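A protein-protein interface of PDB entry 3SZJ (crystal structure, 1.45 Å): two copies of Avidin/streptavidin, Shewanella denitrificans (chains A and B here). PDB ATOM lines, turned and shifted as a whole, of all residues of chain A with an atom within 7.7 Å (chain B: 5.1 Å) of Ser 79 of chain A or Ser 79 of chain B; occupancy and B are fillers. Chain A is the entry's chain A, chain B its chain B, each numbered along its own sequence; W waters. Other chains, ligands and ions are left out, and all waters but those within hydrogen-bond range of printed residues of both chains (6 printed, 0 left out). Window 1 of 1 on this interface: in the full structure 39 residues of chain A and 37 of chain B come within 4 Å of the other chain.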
ATOM      1  N   ASN A  53      -3.292  -9.200  31.315  1.00  0.00           N
ATOM      2  CA  ASN A  53      -2.708  -8.177  32.201  1.00  0.00           C
ATOM      3  C   ASN A  53      -3.827  -7.333  32.824  1.00  0.00           C
ATOM      4  O   ASN A  53      -5.003  -7.499  32.489  1.00  0.00           O
ATOM      5  CB  ASN A  53      -1.620  -7.308  31.511  1.00  0.00           C
ATOM      6  CG  ASN A  53      -2.130  -6.563  30.319  1.00  0.00           C
ATOM      7  OD1 ASN A  53      -3.301  -6.191  30.262  1.00  0.00           O
ATOM      8  ND2 ASN A  53      -1.244  -6.357  29.327  1.00  0.00           N
ATOM      9  N   TRP A  55      -4.991  -4.626  36.507  1.00  0.00           N
ATOM     10  CA  TRP A  55      -4.760  -3.863  37.742  1.00  0.00           C
ATOM     11  C   TRP A  55      -5.723  -4.318  38.833  1.00  0.00           C
ATOM     12  O   TRP A  55      -6.888  -4.616  38.541  1.00  0.00           O
ATOM     13  CB  TRP A  55      -5.054  -2.367  37.520  1.00  0.00           C
ATOM     14  CG  TRP A  55      -4.133  -1.636  36.619  1.00  0.00           C
ATOM     15  CD1 TRP A  55      -4.418  -1.147  35.363  1.00  0.00           C
ATOM     16  CD2 TRP A  55      -2.779  -1.255  36.908  1.00  0.00           C
ATOM     17  NE1 TRP A  55      -3.301  -0.499  34.848  1.00  0.00           N
ATOM     18  CE2 TRP A  55      -2.293  -0.544  35.783  1.00  0.00           C
ATOM     19  CE3 TRP A  55      -1.947  -1.413  38.019  1.00  0.00           C
ATOM     20  CZ2 TRP A  55      -0.991  -0.004  35.731  1.00  0.00           C
ATOM     21  CZ3 TRP A  55      -0.642  -0.879  37.967  1.00  0.00           C
ATOM     22  CH2 TRP A  55      -0.178  -0.202  36.825  1.00  0.00           C
ATOM     23  N   ILE A  61     -11.045  -4.336  40.173  1.00  0.00           N
ATOM     24  CA  ILE A  61     -10.095  -5.082  39.336  1.00  0.00           C
ATOM     25  C   ILE A  61     -10.391  -4.795  37.872  1.00  0.00           C
ATOM     26  O   ILE A  61     -11.553  -4.690  37.477  1.00  0.00           O
ATOM     27  CB  ILE A  61     -10.114  -6.619  39.635  1.00  0.00           C
ATOM     28  CG1 ILE A  61      -9.129  -7.382  38.731  1.00  0.00           C
ATOM     29  CG2 ILE A  61     -11.531  -7.201  39.555  1.00  0.00           C
ATOM     30  CD1 ILE A  61      -8.973  -8.858  39.104  1.00  0.00           C
ATOM     31  N   SER A  62      -9.342  -4.649  37.066  1.00  0.00           N
ATOM     32  CA  SER A  62      -9.500  -4.718  35.611  1.00  0.00           C
ATOM     33  C   SER A  62      -8.559  -5.780  35.090  1.00  0.00           C
ATOM     34  O   SER A  62      -7.462  -5.959  35.626  1.00  0.00           O
ATOM     35  CB  SER A  62      -9.224  -3.371  34.950  1.00  0.00           C
ATOM     36  OG  SER A  62      -7.838  -3.082  34.853  1.00  0.00           O
ATOM     37  N   PHE A  63      -9.005  -6.506  34.068  1.00  0.00           N
ATOM     38  CA  PHE A  63      -8.089  -7.425  33.360  1.00  0.00           C
ATOM     39  C   PHE A  63      -8.471  -7.520  31.883  1.00  0.00           C
ATOM     40  O   PHE A  63      -9.630  -7.304  31.510  1.00  0.00           O
ATOM     41  CB  PHE A  63      -7.969  -8.801  34.071  1.00  0.00           C
ATOM     42  CG  PHE A  63      -9.276  -9.570  34.193  1.00  0.00           C
ATOM     43  CD1 PHE A  63     -10.132  -9.357  35.276  1.00  0.00           C
ATOM     44  CD2 PHE A  63      -9.637 -10.514  33.235  1.00  0.00           C
ATOM     45  CE1 PHE A  63     -11.321 -10.090  35.388  1.00  0.00           C
ATOM     46  CE2 PHE A  63     -10.839 -11.245  33.352  1.00  0.00           C
ATOM     47  CZ  PHE A  63     -11.663 -11.029  34.431  1.00  0.00           C
ATOM     48  N   SER A  64      -7.459  -7.755  31.063  1.00  0.00           N
ATOM     49  CA  SER A  64      -7.632  -7.775  29.622  1.00  0.00           C
ATOM     50  C   SER A  64      -6.837  -8.926  29.021  1.00  0.00           C
ATOM     51  O   SER A  64      -5.712  -9.181  29.437  1.00  0.00           O
ATOM     52  CB  SER A  64      -7.129  -6.449  29.023  1.00  0.00           C
ATOM     53  OG  SER A  64      -7.417  -6.339  27.633  1.00  0.00           O
ATOM     54  N   THR A  65      -7.470  -9.603  28.048  1.00  0.00           N
ATOM     55  CA  THR A  65      -6.869 -10.749  27.364  1.00  0.00           C
ATOM     56  C   THR A  65      -6.761 -10.431  25.874  1.00  0.00           C
ATOM     57  O   THR A  65      -7.722  -9.926  25.268  1.00  0.00           O
ATOM     58  CB  THR A  65      -7.754 -11.985  27.528  1.00  0.00           C
ATOM     59  OG1 THR A  65      -9.049 -11.708  26.999  1.00  0.00           O
ATOM     60  CG2 THR A  65      -7.888 -12.352  28.997  1.00  0.00           C
ATOM     61  N   LYS A  66      -5.586 -10.697  25.291  1.00  0.00           N
ATOM     62  CA  LYS A  66      -5.393 -10.616  23.839  1.00  0.00           C
ATOM     63  C   LYS A  66      -5.538 -12.012  23.251  1.00  0.00           C
ATOM     64  O   LYS A  66      -4.818 -12.937  23.652  1.00  0.00           O
ATOM     65  CB  LYS A  66      -4.020 -10.037  23.486  1.00  0.00           C
ATOM     66  CG  LYS A  66      -3.665 -10.088  21.993  1.00  0.00           C
ATOM     67  CD  LYS A  66      -2.355  -9.358  21.692  1.00  0.00           C
ATOM     68  CE  LYS A  66      -1.942  -9.588  20.260  1.00  0.00           C
ATOM     69  NZ  LYS A  66      -0.765  -8.732  19.921  1.00  0.00           N
ATOM     70  N   TRP A  67      -6.443 -12.146  22.291  1.00  0.00           N
ATOM     71  CA  TRP A  67      -6.819 -13.481  21.798  1.00  0.00           C
ATOM     72  C   TRP A  67      -5.875 -13.957  20.675  1.00  0.00           C
ATOM     73  O   TRP A  67      -6.285 -14.204  19.528  1.00  0.00           O
ATOM     74  CB  TRP A  67      -8.299 -13.493  21.366  1.00  0.00           C
ATOM     75  CG  TRP A  67      -9.237 -13.164  22.510  1.00  0.00           C
ATOM     76  CD1 TRP A  67      -9.940 -11.980  22.705  1.00  0.00           C
ATOM     77  CD2 TRP A  67      -9.588 -14.020  23.613  1.00  0.00           C
ATOM     78  NE1 TRP A  67     -10.661 -12.051  23.867  1.00  0.00           N
ATOM     79  CE2 TRP A  67     -10.490 -13.292  24.433  1.00  0.00           C
ATOM     80  CE3 TRP A  67      -9.247 -15.328  23.981  1.00  0.00           C
ATOM     81  CZ2 TRP A  67     -11.035 -13.826  25.606  1.00  0.00           C
ATOM     82  CZ3 TRP A  67      -9.783 -15.853  25.145  1.00  0.00           C
ATOM     83  CH2 TRP A  67     -10.667 -15.105  25.943  1.00  0.00           C
ATOM     84  N   ILE A  77      -9.465  -8.378  21.348  1.00  0.00           N
ATOM     85  CA  ILE A  77      -9.039  -8.137  22.735  1.00  0.00           C
ATOM     86  C   ILE A  77     -10.284  -7.949  23.612  1.00  0.00           C
ATOM     87  O   ILE A  77     -11.181  -7.180  23.255  1.00  0.00           O
ATOM     88  CB  ILE A  77      -8.182  -6.848  22.853  1.00  0.00           C
ATOM     89  CG1 ILE A  77      -6.930  -6.900  21.979  1.00  0.00           C
ATOM     90  CG2 ILE A  77      -7.775  -6.588  24.310  1.00  0.00           C
ATOM     91  CD1 ILE A  77      -6.295  -5.540  21.760  1.00  0.00           C
ATOM     92  N   THR A  78     -10.373  -8.675  24.737  1.00  0.00           N
ATOM     93  CA  THR A  78     -11.451  -8.424  25.718  1.00  0.00           C
ATOM     94  C   THR A  78     -10.896  -7.718  26.949  1.00  0.00           C
ATOM     95  O   THR A  78      -9.790  -8.022  27.393  1.00  0.00           O
ATOM     96  CB  THR A  78     -12.145  -9.731  26.130  1.00  0.00           C
ATOM     97  OG1 THR A  78     -12.640 -10.339  24.938  1.00  0.00           O
ATOM     98  CG2 THR A  78     -13.342  -9.446  27.069  1.00  0.00           C
ATOM     99  N   SER A  79     -11.672  -6.755  27.450  1.00  0.00           N
ATOM    100  CA  SER A  79     -11.374  -6.038  28.681  1.00  0.00           C
ATOM    101  C   SER A  79     -12.529  -6.232  29.658  1.00  0.00           C
ATOM    102  O   SER A  79     -13.678  -6.009  29.296  1.00  0.00           O
ATOM    103  CB  SER A  79     -11.222  -4.548  28.359  1.00  0.00           C
ATOM    104  OG  SER A  79     -11.030  -3.761  29.515  1.00  0.00           O
ATOM    105  N   TRP A  80     -12.208  -6.630  30.886  1.00  0.00           N
ATOM    106  CA  TRP A  80     -13.191  -6.726  31.960  1.00  0.00           C
ATOM    107  C   TRP A  80     -12.909  -5.656  33.014  1.00  0.00           C
ATOM    108  O   TRP A  80     -11.737  -5.401  33.370  1.00  0.00           O
ATOM    109  CB  TRP A  80     -13.081  -8.079  32.663  1.00  0.00           C
ATOM    110  CG  TRP A  80     -13.529  -9.336  31.913  1.00  0.00           C
ATOM    111  CD1 TRP A  80     -14.726 -10.004  32.063  1.00  0.00           C
ATOM    112  CD2 TRP A  80     -12.762 -10.094  30.950  1.00  0.00           C
ATOM    113  NE1 TRP A  80     -14.746 -11.137  31.248  1.00  0.00           N
ATOM    114  CE2 TRP A  80     -13.553 -11.210  30.565  1.00  0.00           C
ATOM    115  CE3 TRP A  80     -11.464  -9.949  30.400  1.00  0.00           C
ATOM    116  CZ2 TRP A  80     -13.081 -12.176  29.659  1.00  0.00           C
ATOM    117  CZ3 TRP A  80     -11.011 -10.897  29.481  1.00  0.00           C
ATOM    118  CH2 TRP A  80     -11.808 -11.998  29.128  1.00  0.00           C
ATOM    119  N   SER A  81     -13.984  -5.060  33.544  1.00  0.00           N
ATOM    120  CA  SER A  81     -13.899  -4.172  34.714  1.00  0.00           C
ATOM    121  C   SER A  81     -14.849  -4.741  35.751  1.00  0.00           C
ATOM    122  O   SER A  81     -15.984  -5.079  35.413  1.00  0.00           O
ATOM    123  CB  SER A  81     -14.366  -2.758  34.359  1.00  0.00           C
ATOM    124  OG  SER A  81     -13.592  -2.211  33.315  1.00  0.00           O
ATOM    125  N   GLY A  82     -14.427  -4.818  37.009  1.00  0.00           N
ATOM    126  CA  GLY A  82     -15.351  -5.358  37.994  1.00  0.00           C
ATOM    127  C   GLY A  82     -14.870  -5.219  39.410  1.00  0.00           C
ATOM    128  O   GLY A  82     -13.946  -4.477  39.704  1.00  0.00           O
ATOM    129  N   THR A  95     -18.281  -8.623  36.938  1.00  0.00           N
ATOM    130  CA  THR A  95     -17.624  -7.812  35.901  1.00  0.00           C
ATOM    131  C   THR A  95     -18.571  -7.422  34.766  1.00  0.00           C
ATOM    132  O   THR A  95     -19.614  -8.081  34.530  1.00  0.00           O
ATOM    133  CB  THR A  95     -16.448  -8.577  35.218  1.00  0.00           C
ATOM    134  OG1 THR A  95     -16.967  -9.622  34.389  1.00  0.00           O
ATOM    135  CG2 THR A  95     -15.433  -9.135  36.238  1.00  0.00           C
ATOM    136  N   LEU A  96     -18.180  -6.362  34.052  1.00  0.00           N
ATOM    137  CA  LEU A  96     -18.756  -6.032  32.746  1.00  0.00           C
ATOM    138  C   LEU A  96     -17.590  -6.069  31.771  1.00  0.00           C
ATOM    139  O   LEU A  96     -16.485  -5.580  32.075  1.00  0.00           O
ATOM    140  CB  LEU A  96     -19.372  -4.644  32.752  1.00  0.00           C
ATOM    141  CG  LEU A  96     -20.552  -4.483  33.717  1.00  0.00           C
ATOM    142  CD1 LEU A  96     -21.021  -3.047  33.652  1.00  0.00           C
ATOM    143  CD2 LEU A  96     -21.704  -5.449  33.343  1.00  0.00           C
ATOM    144  N   TRP A  97     -17.817  -6.637  30.591  1.00  0.00           N
ATOM    145  CA  TRP A  97     -16.728  -6.742  29.596  1.00  0.00           C
ATOM    146  C   TRP A  97     -17.031  -6.074  28.259  1.00  0.00           C
ATOM    147  O   TRP A  97     -18.201  -5.863  27.898  1.00  0.00           O
ATOM    148  CB  TRP A  97     -16.296  -8.187  29.344  1.00  0.00           C
ATOM    149  CG  TRP A  97     -17.384  -9.167  28.940  1.00  0.00           C
ATOM    150  CD1 TRP A  97     -18.068 -10.013  29.762  1.00  0.00           C
ATOM    151  CD2 TRP A  97     -17.884  -9.393  27.613  1.00  0.00           C
ATOM    152  NE1 TRP A  97     -18.993 -10.735  29.029  1.00  0.00           N
ATOM    153  CE2 TRP A  97     -18.891 -10.385  27.705  1.00  0.00           C
ATOM    154  CE3 TRP A  97     -17.565  -8.856  26.350  1.00  0.00           C
ATOM    155  CZ2 TRP A  97     -19.590 -10.862  26.575  1.00  0.00           C
ATOM    156  CZ3 TRP A  97     -18.258  -9.305  25.243  1.00  0.00           C
ATOM    157  CH2 TRP A  97     -19.271 -10.306  25.360  1.00  0.00           C
ATOM    158  N   GLN A  98     -15.951  -5.787  27.514  1.00  0.00           N
ATOM    159  CA  GLN A  98     -16.002  -5.200  26.187  1.00  0.00           C
ATOM    160  C   GLN A  98     -15.019  -5.975  25.317  1.00  0.00           C
ATOM    161  O   GLN A  98     -13.894  -6.231  25.744  1.00  0.00           O
ATOM    162  CB  GLN A  98     -15.582  -3.720  26.241  1.00  0.00           C
ATOM    163  CG  GLN A  98     -16.496  -2.871  27.099  1.00  0.00           C
ATOM    164  CD  GLN A  98     -16.218  -1.369  26.982  1.00  0.00           C
ATOM    165  OE1 GLN A  98     -15.065  -0.933  26.947  1.00  0.00           O
ATOM    166  NE2 GLN A  98     -17.276  -0.586  27.010  1.00  0.00           N
ATOM    167  N   LEU A  99     -15.424  -6.298  24.085  1.00  0.00           N
ATOM    168  CA  LEU A  99     -14.589  -7.054  23.155  1.00  0.00           C
ATOM    169  C   LEU A  99     -14.455  -6.228  21.878  1.00  0.00           C
ATOM    170  O   LEU A  99     -15.460  -5.896  21.258  1.00  0.00           O
ATOM    171  CB  LEU A  99     -15.247  -8.423  22.884  1.00  0.00           C
ATOM    172  CG  LEU A  99     -14.798  -9.448  21.829  1.00  0.00           C
ATOM    173  CD1 LEU A  99     -13.321  -9.760  21.847  1.00  0.00           C
ATOM    174  CD2 LEU A  99     -15.585 -10.746  22.020  1.00  0.00           C
ATOM    175  N   VAL A 100     -13.217  -5.887  21.519  1.00  0.00           N
ATOM    176  CA  VAL A 100     -12.948  -5.093  20.317  1.00  0.00           C
ATOM    177  C   VAL A 100     -12.144  -5.922  19.303  1.00  0.00           C
ATOM    178  O   VAL A 100     -11.222  -6.644  19.680  1.00  0.00           O
ATOM    179  CB  VAL A 100     -12.216  -3.742  20.632  1.00  0.00           C
ATOM    180  CG1 VAL A 100     -10.857  -3.963  21.331  1.00  0.00           C
ATOM    181  CG2 VAL A 100     -12.106  -2.859  19.349  1.00  0.00           C
ATOM    182  N   LEU A 111     -18.395  -5.513  21.210  1.00  0.00           N
ATOM    183  CA  LEU A 111     -19.355  -6.376  21.904  1.00  0.00           C
ATOM    184  C   LEU A 111     -19.286  -6.156  23.418  1.00  0.00           C
ATOM    185  O   LEU A 111     -18.225  -5.813  23.964  1.00  0.00           O
ATOM    186  CB  LEU A 111     -19.089  -7.857  21.572  1.00  0.00           C
ATOM    187  CG  LEU A 111     -19.006  -8.250  20.092  1.00  0.00           C
ATOM    188  CD1 LEU A 111     -18.730  -9.754  19.904  1.00  0.00           C
ATOM    189  CD2 LEU A 111     -20.279  -7.845  19.364  1.00  0.00           C
ATOM    190  N   GLY A 113     -20.895  -7.427  27.504  1.00  0.00           N
ATOM    191  CA  GLY A 113     -21.611  -8.419  28.317  1.00  0.00           C
ATOM    192  C   GLY A 113     -21.215  -8.377  29.772  1.00  0.00           C
ATOM    193  O   GLY A 113     -20.472  -7.492  30.189  1.00  0.00           O
ATOM    194  N   SER B  62      -6.548  -2.158  23.746  1.00  0.00           N
ATOM    195  CA  SER B  62      -7.112  -1.911  25.084  1.00  0.00           C
ATOM    196  C   SER B  62      -6.051  -1.258  25.953  1.00  0.00           C
ATOM    197  O   SER B  62      -4.852  -1.556  25.820  1.00  0.00           O
ATOM    198  CB  SER B  62      -7.604  -3.188  25.774  1.00  0.00           C
ATOM    199  OG  SER B  62      -6.540  -4.006  26.222  1.00  0.00           O
ATOM    200  N   PHE B  63      -6.476  -0.363  26.836  1.00  0.00           N
ATOM    201  CA  PHE B  63      -5.527   0.169  27.815  1.00  0.00           C
ATOM    202  C   PHE B  63      -6.253   0.470  29.107  1.00  0.00           C
ATOM    203  O   PHE B  63      -7.457   0.738  29.107  1.00  0.00           O
ATOM    204  CB  PHE B  63      -4.675   1.356  27.261  1.00  0.00           C
ATOM    205  CG  PHE B  63      -5.468   2.555  26.814  1.00  0.00           C
ATOM    206  CD1 PHE B  63      -5.986   2.628  25.515  1.00  0.00           C
ATOM    207  CD2 PHE B  63      -5.665   3.638  27.672  1.00  0.00           C
ATOM    208  CE1 PHE B  63      -6.721   3.763  25.090  1.00  0.00           C
ATOM    209  CE2 PHE B  63      -6.362   4.780  27.241  1.00  0.00           C
ATOM    210  CZ  PHE B  63      -6.882   4.841  25.963  1.00  0.00           C
ATOM    211  N   SER B  64      -5.523   0.410  30.205  1.00  0.00           N
ATOM    212  CA  SER B  64      -6.157   0.552  31.508  1.00  0.00           C
ATOM    213  C   SER B  64      -5.219   1.336  32.436  1.00  0.00           C
ATOM    214  O   SER B  64      -3.997   1.128  32.432  1.00  0.00           O
ATOM    215  CB  SER B  64      -6.451  -0.830  32.119  1.00  0.00           C
ATOM    216  OG  SER B  64      -7.152  -0.734  33.364  1.00  0.00           O
ATOM    217  N   ILE B  77     -10.238   2.396  38.822  1.00  0.00           N
ATOM    218  CA  ILE B  77      -9.504   1.918  37.635  1.00  0.00           C
ATOM    219  C   ILE B  77     -10.353   2.180  36.398  1.00  0.00           C
ATOM    220  O   ILE B  77     -11.553   1.893  36.406  1.00  0.00           O
ATOM    221  CB  ILE B  77      -9.224   0.380  37.692  1.00  0.00           C
ATOM    222  CG1 ILE B  77      -8.446   0.005  38.949  1.00  0.00           C
ATOM    223  CG2 ILE B  77      -8.432  -0.046  36.451  1.00  0.00           C
ATOM    224  CD1 ILE B  77      -8.465  -1.495  39.233  1.00  0.00           C
ATOM    225  N   THR B  78      -9.753   2.740  35.344  1.00  0.00           N
ATOM    226  CA  THR B  78     -10.465   2.894  34.076  1.00  0.00           C
ATOM    227  C   THR B  78      -9.884   1.966  33.027  1.00  0.00           C
ATOM    228  O   THR B  78      -8.680   1.741  32.975  1.00  0.00           O
ATOM    229  CB  THR B  78     -10.399   4.339  33.550  1.00  0.00           C
ATOM    230  OG1 THR B  78     -11.011   5.179  34.529  1.00  0.00           O
ATOM    231  CG2 THR B  78     -11.180   4.502  32.240  1.00  0.00           C
ATOM    232  N   SER B  79     -10.766   1.403  32.215  1.00  0.00           N
ATOM    233  CA  SER B  79     -10.306   0.601  31.095  1.00  0.00           C
ATOM    234  C   SER B  79     -10.979   1.065  29.824  1.00  0.00           C
ATOM    235  O   SER B  79     -12.187   1.283  29.792  1.00  0.00           O
ATOM    236  CB  SER B  79     -10.598  -0.871  31.323  1.00  0.00           C
ATOM    237  OG  SER B  79     -11.984  -1.107  31.348  1.00  0.00           O
ATOM    238  N   TRP B  80     -10.165   1.229  28.792  1.00  0.00           N
ATOM    239  CA  TRP B  80     -10.666   1.618  27.489  1.00  0.00           C
ATOM    240  C   TRP B  80     -10.497   0.467  26.512  1.00  0.00           C
ATOM    241  O   TRP B  80      -9.475  -0.257  26.542  1.00  0.00           O
ATOM    242  CB  TRP B  80      -9.843   2.789  26.942  1.00  0.00           C
ATOM    243  CG  TRP B  80      -9.938   4.144  27.602  1.00  0.00           C
ATOM    244  CD1 TRP B  80     -10.630   5.243  27.126  1.00  0.00           C
ATOM    245  CD2 TRP B  80      -9.268   4.578  28.795  1.00  0.00           C
ATOM    246  NE1 TRP B  80     -10.427   6.329  27.961  1.00  0.00           N
ATOM    247  CE2 TRP B  80      -9.603   5.942  28.995  1.00  0.00           C
ATOM    248  CE3 TRP B  80      -8.398   3.957  29.703  1.00  0.00           C
ATOM    249  CZ2 TRP B  80      -9.068   6.691  30.069  1.00  0.00           C
ATOM    250  CZ3 TRP B  80      -7.884   4.697  30.771  1.00  0.00           C
ATOM    251  CH2 TRP B  80      -8.215   6.044  30.942  1.00  0.00           C
ATOM    252  N   SER B  81     -11.492   0.309  25.639  1.00  0.00           N
ATOM    253  CA  SER B  81     -11.402  -0.640  24.520  1.00  0.00           C
ATOM    254  C   SER B  81     -11.606   0.175  23.265  1.00  0.00           C
ATOM    255  O   SER B  81     -12.556   0.968  23.206  1.00  0.00           O
ATOM    256  CB  SER B  81     -12.517  -1.684  24.604  1.00  0.00           C
ATOM    257  OG  SER B  81     -12.410  -2.442  25.792  1.00  0.00           O
ATOM    258  N   LEU B  96     -14.482   3.098  23.869  1.00  0.00           N
ATOM    259  CA  LEU B  96     -15.504   3.094  24.922  1.00  0.00           C
ATOM    260  C   LEU B  96     -14.797   2.716  26.205  1.00  0.00           C
ATOM    261  O   LEU B  96     -13.927   1.811  26.199  1.00  0.00           O
ATOM    262  CB  LEU B  96     -16.596   2.072  24.632  1.00  0.00           C
ATOM    263  CG  LEU B  96     -17.365   2.239  23.308  1.00  0.00           C
ATOM    264  CD1 LEU B  96     -18.330   1.063  23.160  1.00  0.00           C
ATOM    265  CD2 LEU B  96     -18.106   3.603  23.242  1.00  0.00           C
ATOM    266  N   TRP B  97     -15.120   3.407  27.293  1.00  0.00           N
ATOM    267  CA  TRP B  97     -14.435   3.113  28.561  1.00  0.00           C
ATOM    268  C   TRP B  97     -15.391   2.749  29.708  1.00  0.00           C
ATOM    269  O   TRP B  97     -16.572   3.106  29.673  1.00  0.00           O
ATOM    270  CB  TRP B  97     -13.507   4.259  29.002  1.00  0.00           C
ATOM    271  CG  TRP B  97     -14.149   5.625  29.115  1.00  0.00           C
ATOM    272  CD1 TRP B  97     -14.113   6.602  28.177  1.00  0.00           C
ATOM    273  CD2 TRP B  97     -14.897   6.151  30.225  1.00  0.00           C
ATOM    274  NE1 TRP B  97     -14.772   7.727  28.639  1.00  0.00           N
ATOM    275  CE2 TRP B  97     -15.295   7.460  29.879  1.00  0.00           C
ATOM    276  CE3 TRP B  97     -15.301   5.630  31.456  1.00  0.00           C
ATOM    277  CZ2 TRP B  97     -16.052   8.267  30.739  1.00  0.00           C
ATOM    278  CZ3 TRP B  97     -16.045   6.432  32.311  1.00  0.00           C
ATOM    279  CH2 TRP B  97     -16.421   7.730  31.948  1.00  0.00           C
ATOM    280  N   GLN B  98     -14.841   2.056  30.715  1.00  0.00           N
ATOM    281  CA  GLN B  98     -15.543   1.674  31.926  1.00  0.00           C
ATOM    282  C   GLN B  98     -14.675   2.054  33.113  1.00  0.00           C
ATOM    283  O   GLN B  98     -13.459   1.802  33.097  1.00  0.00           O
ATOM    284  CB  GLN B  98     -15.786   0.156  31.946  1.00  0.00           C
ATOM    285  CG  GLN B  98     -16.658  -0.308  30.795  1.00  0.00           C
ATOM    286  CD  GLN B  98     -16.969  -1.771  30.830  1.00  0.00           C
ATOM    287  OE1 GLN B  98     -16.119  -2.604  31.185  1.00  0.00           O
ATOM    288  NE2 GLN B  98     -18.181  -2.104  30.448  1.00  0.00           N
ATOM    289  N   LEU B  99     -15.299   2.615  34.155  1.00  0.00           N
ATOM    290  CA  LEU B  99     -14.582   3.064  35.344  1.00  0.00           C
ATOM    291  C   LEU B  99     -15.168   2.339  36.542  1.00  0.00           C
ATOM    292  O   LEU B  99     -16.363   2.470  36.791  1.00  0.00           O
ATOM    293  CB  LEU B  99     -14.749   4.587  35.488  1.00  0.00           C
ATOM    294  CG  LEU B  99     -14.307   5.360  36.733  1.00  0.00           C
ATOM    295  CD1 LEU B  99     -12.916   4.985  37.173  1.00  0.00           C
ATOM    296  CD2 LEU B  99     -14.366   6.848  36.433  1.00  0.00           C
HETATM  297  O   HOH W   1     -10.938  -4.514  25.088  1.00  0.00           O
HETATM  298  O   HOH W   2     -18.379   1.751  27.866  1.00  0.00           O
HETATM  299  O   HOH W   3     -11.788  -0.751  34.667  1.00  0.00           O
HETATM  300  O   HOH W   4      -8.982  -2.140  28.769  1.00  0.00           O
HETATM  301  O   HOH W   5     -13.647  -3.001  30.499  1.00  0.00           O
HETATM  302  O   HOH W   6     -19.741  -3.793  29.013  1.00  0.00           O
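The indole nitrogen (NE1) of Trp 55 of chain A lies within hydrogen-bond range of the backbone carbonyl oxygen (O) of Ser 64 of chain B (3.0 Å). OG of Ser 64 of chain B lies within hydrogen-bond range of OG of Ser 62 of chain A. The side-chain hydroxyl (OG) of Ser 64 of chain A is in hydrogen-bond range of the side-chain hydroxyl (OG) of Ser 62 of chain B (2.9 Å). The side-chain hydroxyl of Ser 79 of chain B sits at hydrogen-bond distance from the side-chain hydroxyl of Ser 79 of chain A (3.4 Å). The side-chain hydroxyl of Ser 81 of chain A lies within hydrogen-bond range of the side-chain hydroxyl of Ser 79 of chain B, at 2.8 Å. The side-chain hydroxyl (OG) of Ser 81 of chain A is in hydrogen-bond range of the side-chain amide oxygen (OE1) of Gln 98 of chain B, at 3.3 Å. The backbone carbonyl oxygen of Leu 96 of chain A sits close to the side-chain amide oxygen of Gln 98 of chain B (3.1 Å). The side-chain amide oxygen of Gln 98 of chain A sits at hydrogen-bond distance from the side-chain hydroxyl of Ser 81 of chain B (3.3 Å). The backbone carbonyl oxygen (O) of Leu 96 of chain B sits close to the side-chain amide oxygen (OE1) of Gln 98 of chain A, 3.1 Å away.
Hydrophobic or aromatic side chains of chain A that line the printed part of chain B: Trp 55, Ile 77 and Leu 96. Among the printed residues, no Asp or Glu carboxylate lies within 4 Å of a Lys or Arg side-chain nitrogen of the other chain.
O of Ile 61 of chain A is in hydrogen-bond range of N of Gly 82 of chain A. The backbone carbonyl oxygen (O) of Ile 77 of chain A is in hydrogen-bond range of the backbone NH (N) of Val 100 of chain A (3.0 Å). N of Ser 79 of chain A is in hydrogen-bond range of O of Gln 98 of chain A, at 2.8 Å. The backbone carbonyl oxygen (O) of Thr 78 of chain B lies within hydrogen-bond range of the side-chain hydroxyl (OG) of Ser 64 of chain B (2.9 Å). N of Ser 79 of chain B is in hydrogen-bond range of O of Gln 98 of chain B (2.9 Å).
Trp 55 of chain A touches Ile 77 of chain B (O to CD1, 3.6 Å). CA of Ile 61 of chain A touches CD1 of Ile 77 of chain B, at 3.9 Å. OG of Ser 62 of chain A touches CG2 of Ile 77 of chain B (3.5 Å). Ser 62 of chain B touches Ile 77 of chain A. Ser 79 of chain A touches Ser 81 of chain B. Gln 98 of chain B touches Gln 98 of chain A.
Water W3 lies within hydrogen-bond range of OG of Ser 81 of chain A (2.7 Å), O of Ile 77 of chain B (3.2 Å), OG of Ser 79 of chain B (3.3 Å) and O of Gln 98 of chain B (3.4 Å). Water W4 lies within hydrogen-bond range of OG of Ser 79 of chain A, O of Trp 80 of chain B and O of Phe 63 of chain B.
Ser 79 of chain A touches its own counterpart, Ser 79 of chain B. Ser 81 of chain A touches Gln 98 of chain B, and with the chains exchanged Gln 98 of chain A touches Ser 81 of chain B. Leu 96 of chain A touches Gln 98 of chain B, and with the chains exchanged Gln 98 of chain A touches Leu 96 of chain B. Gln 98 of chain B touches its own counterpart, Gln 98 of chain A.
Printed residues of chain B within 4 Å of Ser 79 of chain A: Ser 79 and Ser 81. Of the printed residues of chain B, Ser 81 of chain A touches Ser 79 and Gln 98. Of the printed residues of chain B, Trp 55 of chain A touches Ser 64 (3.0 Å) and Ile 77 (3.6 Å). Of the printed residues of chain B, Ile 77 of chain A touches Ser 62. The nearest printed residue of chain A that does not touch Ser 79 of chain B is Gln 98 of chain A (4.6 Å).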
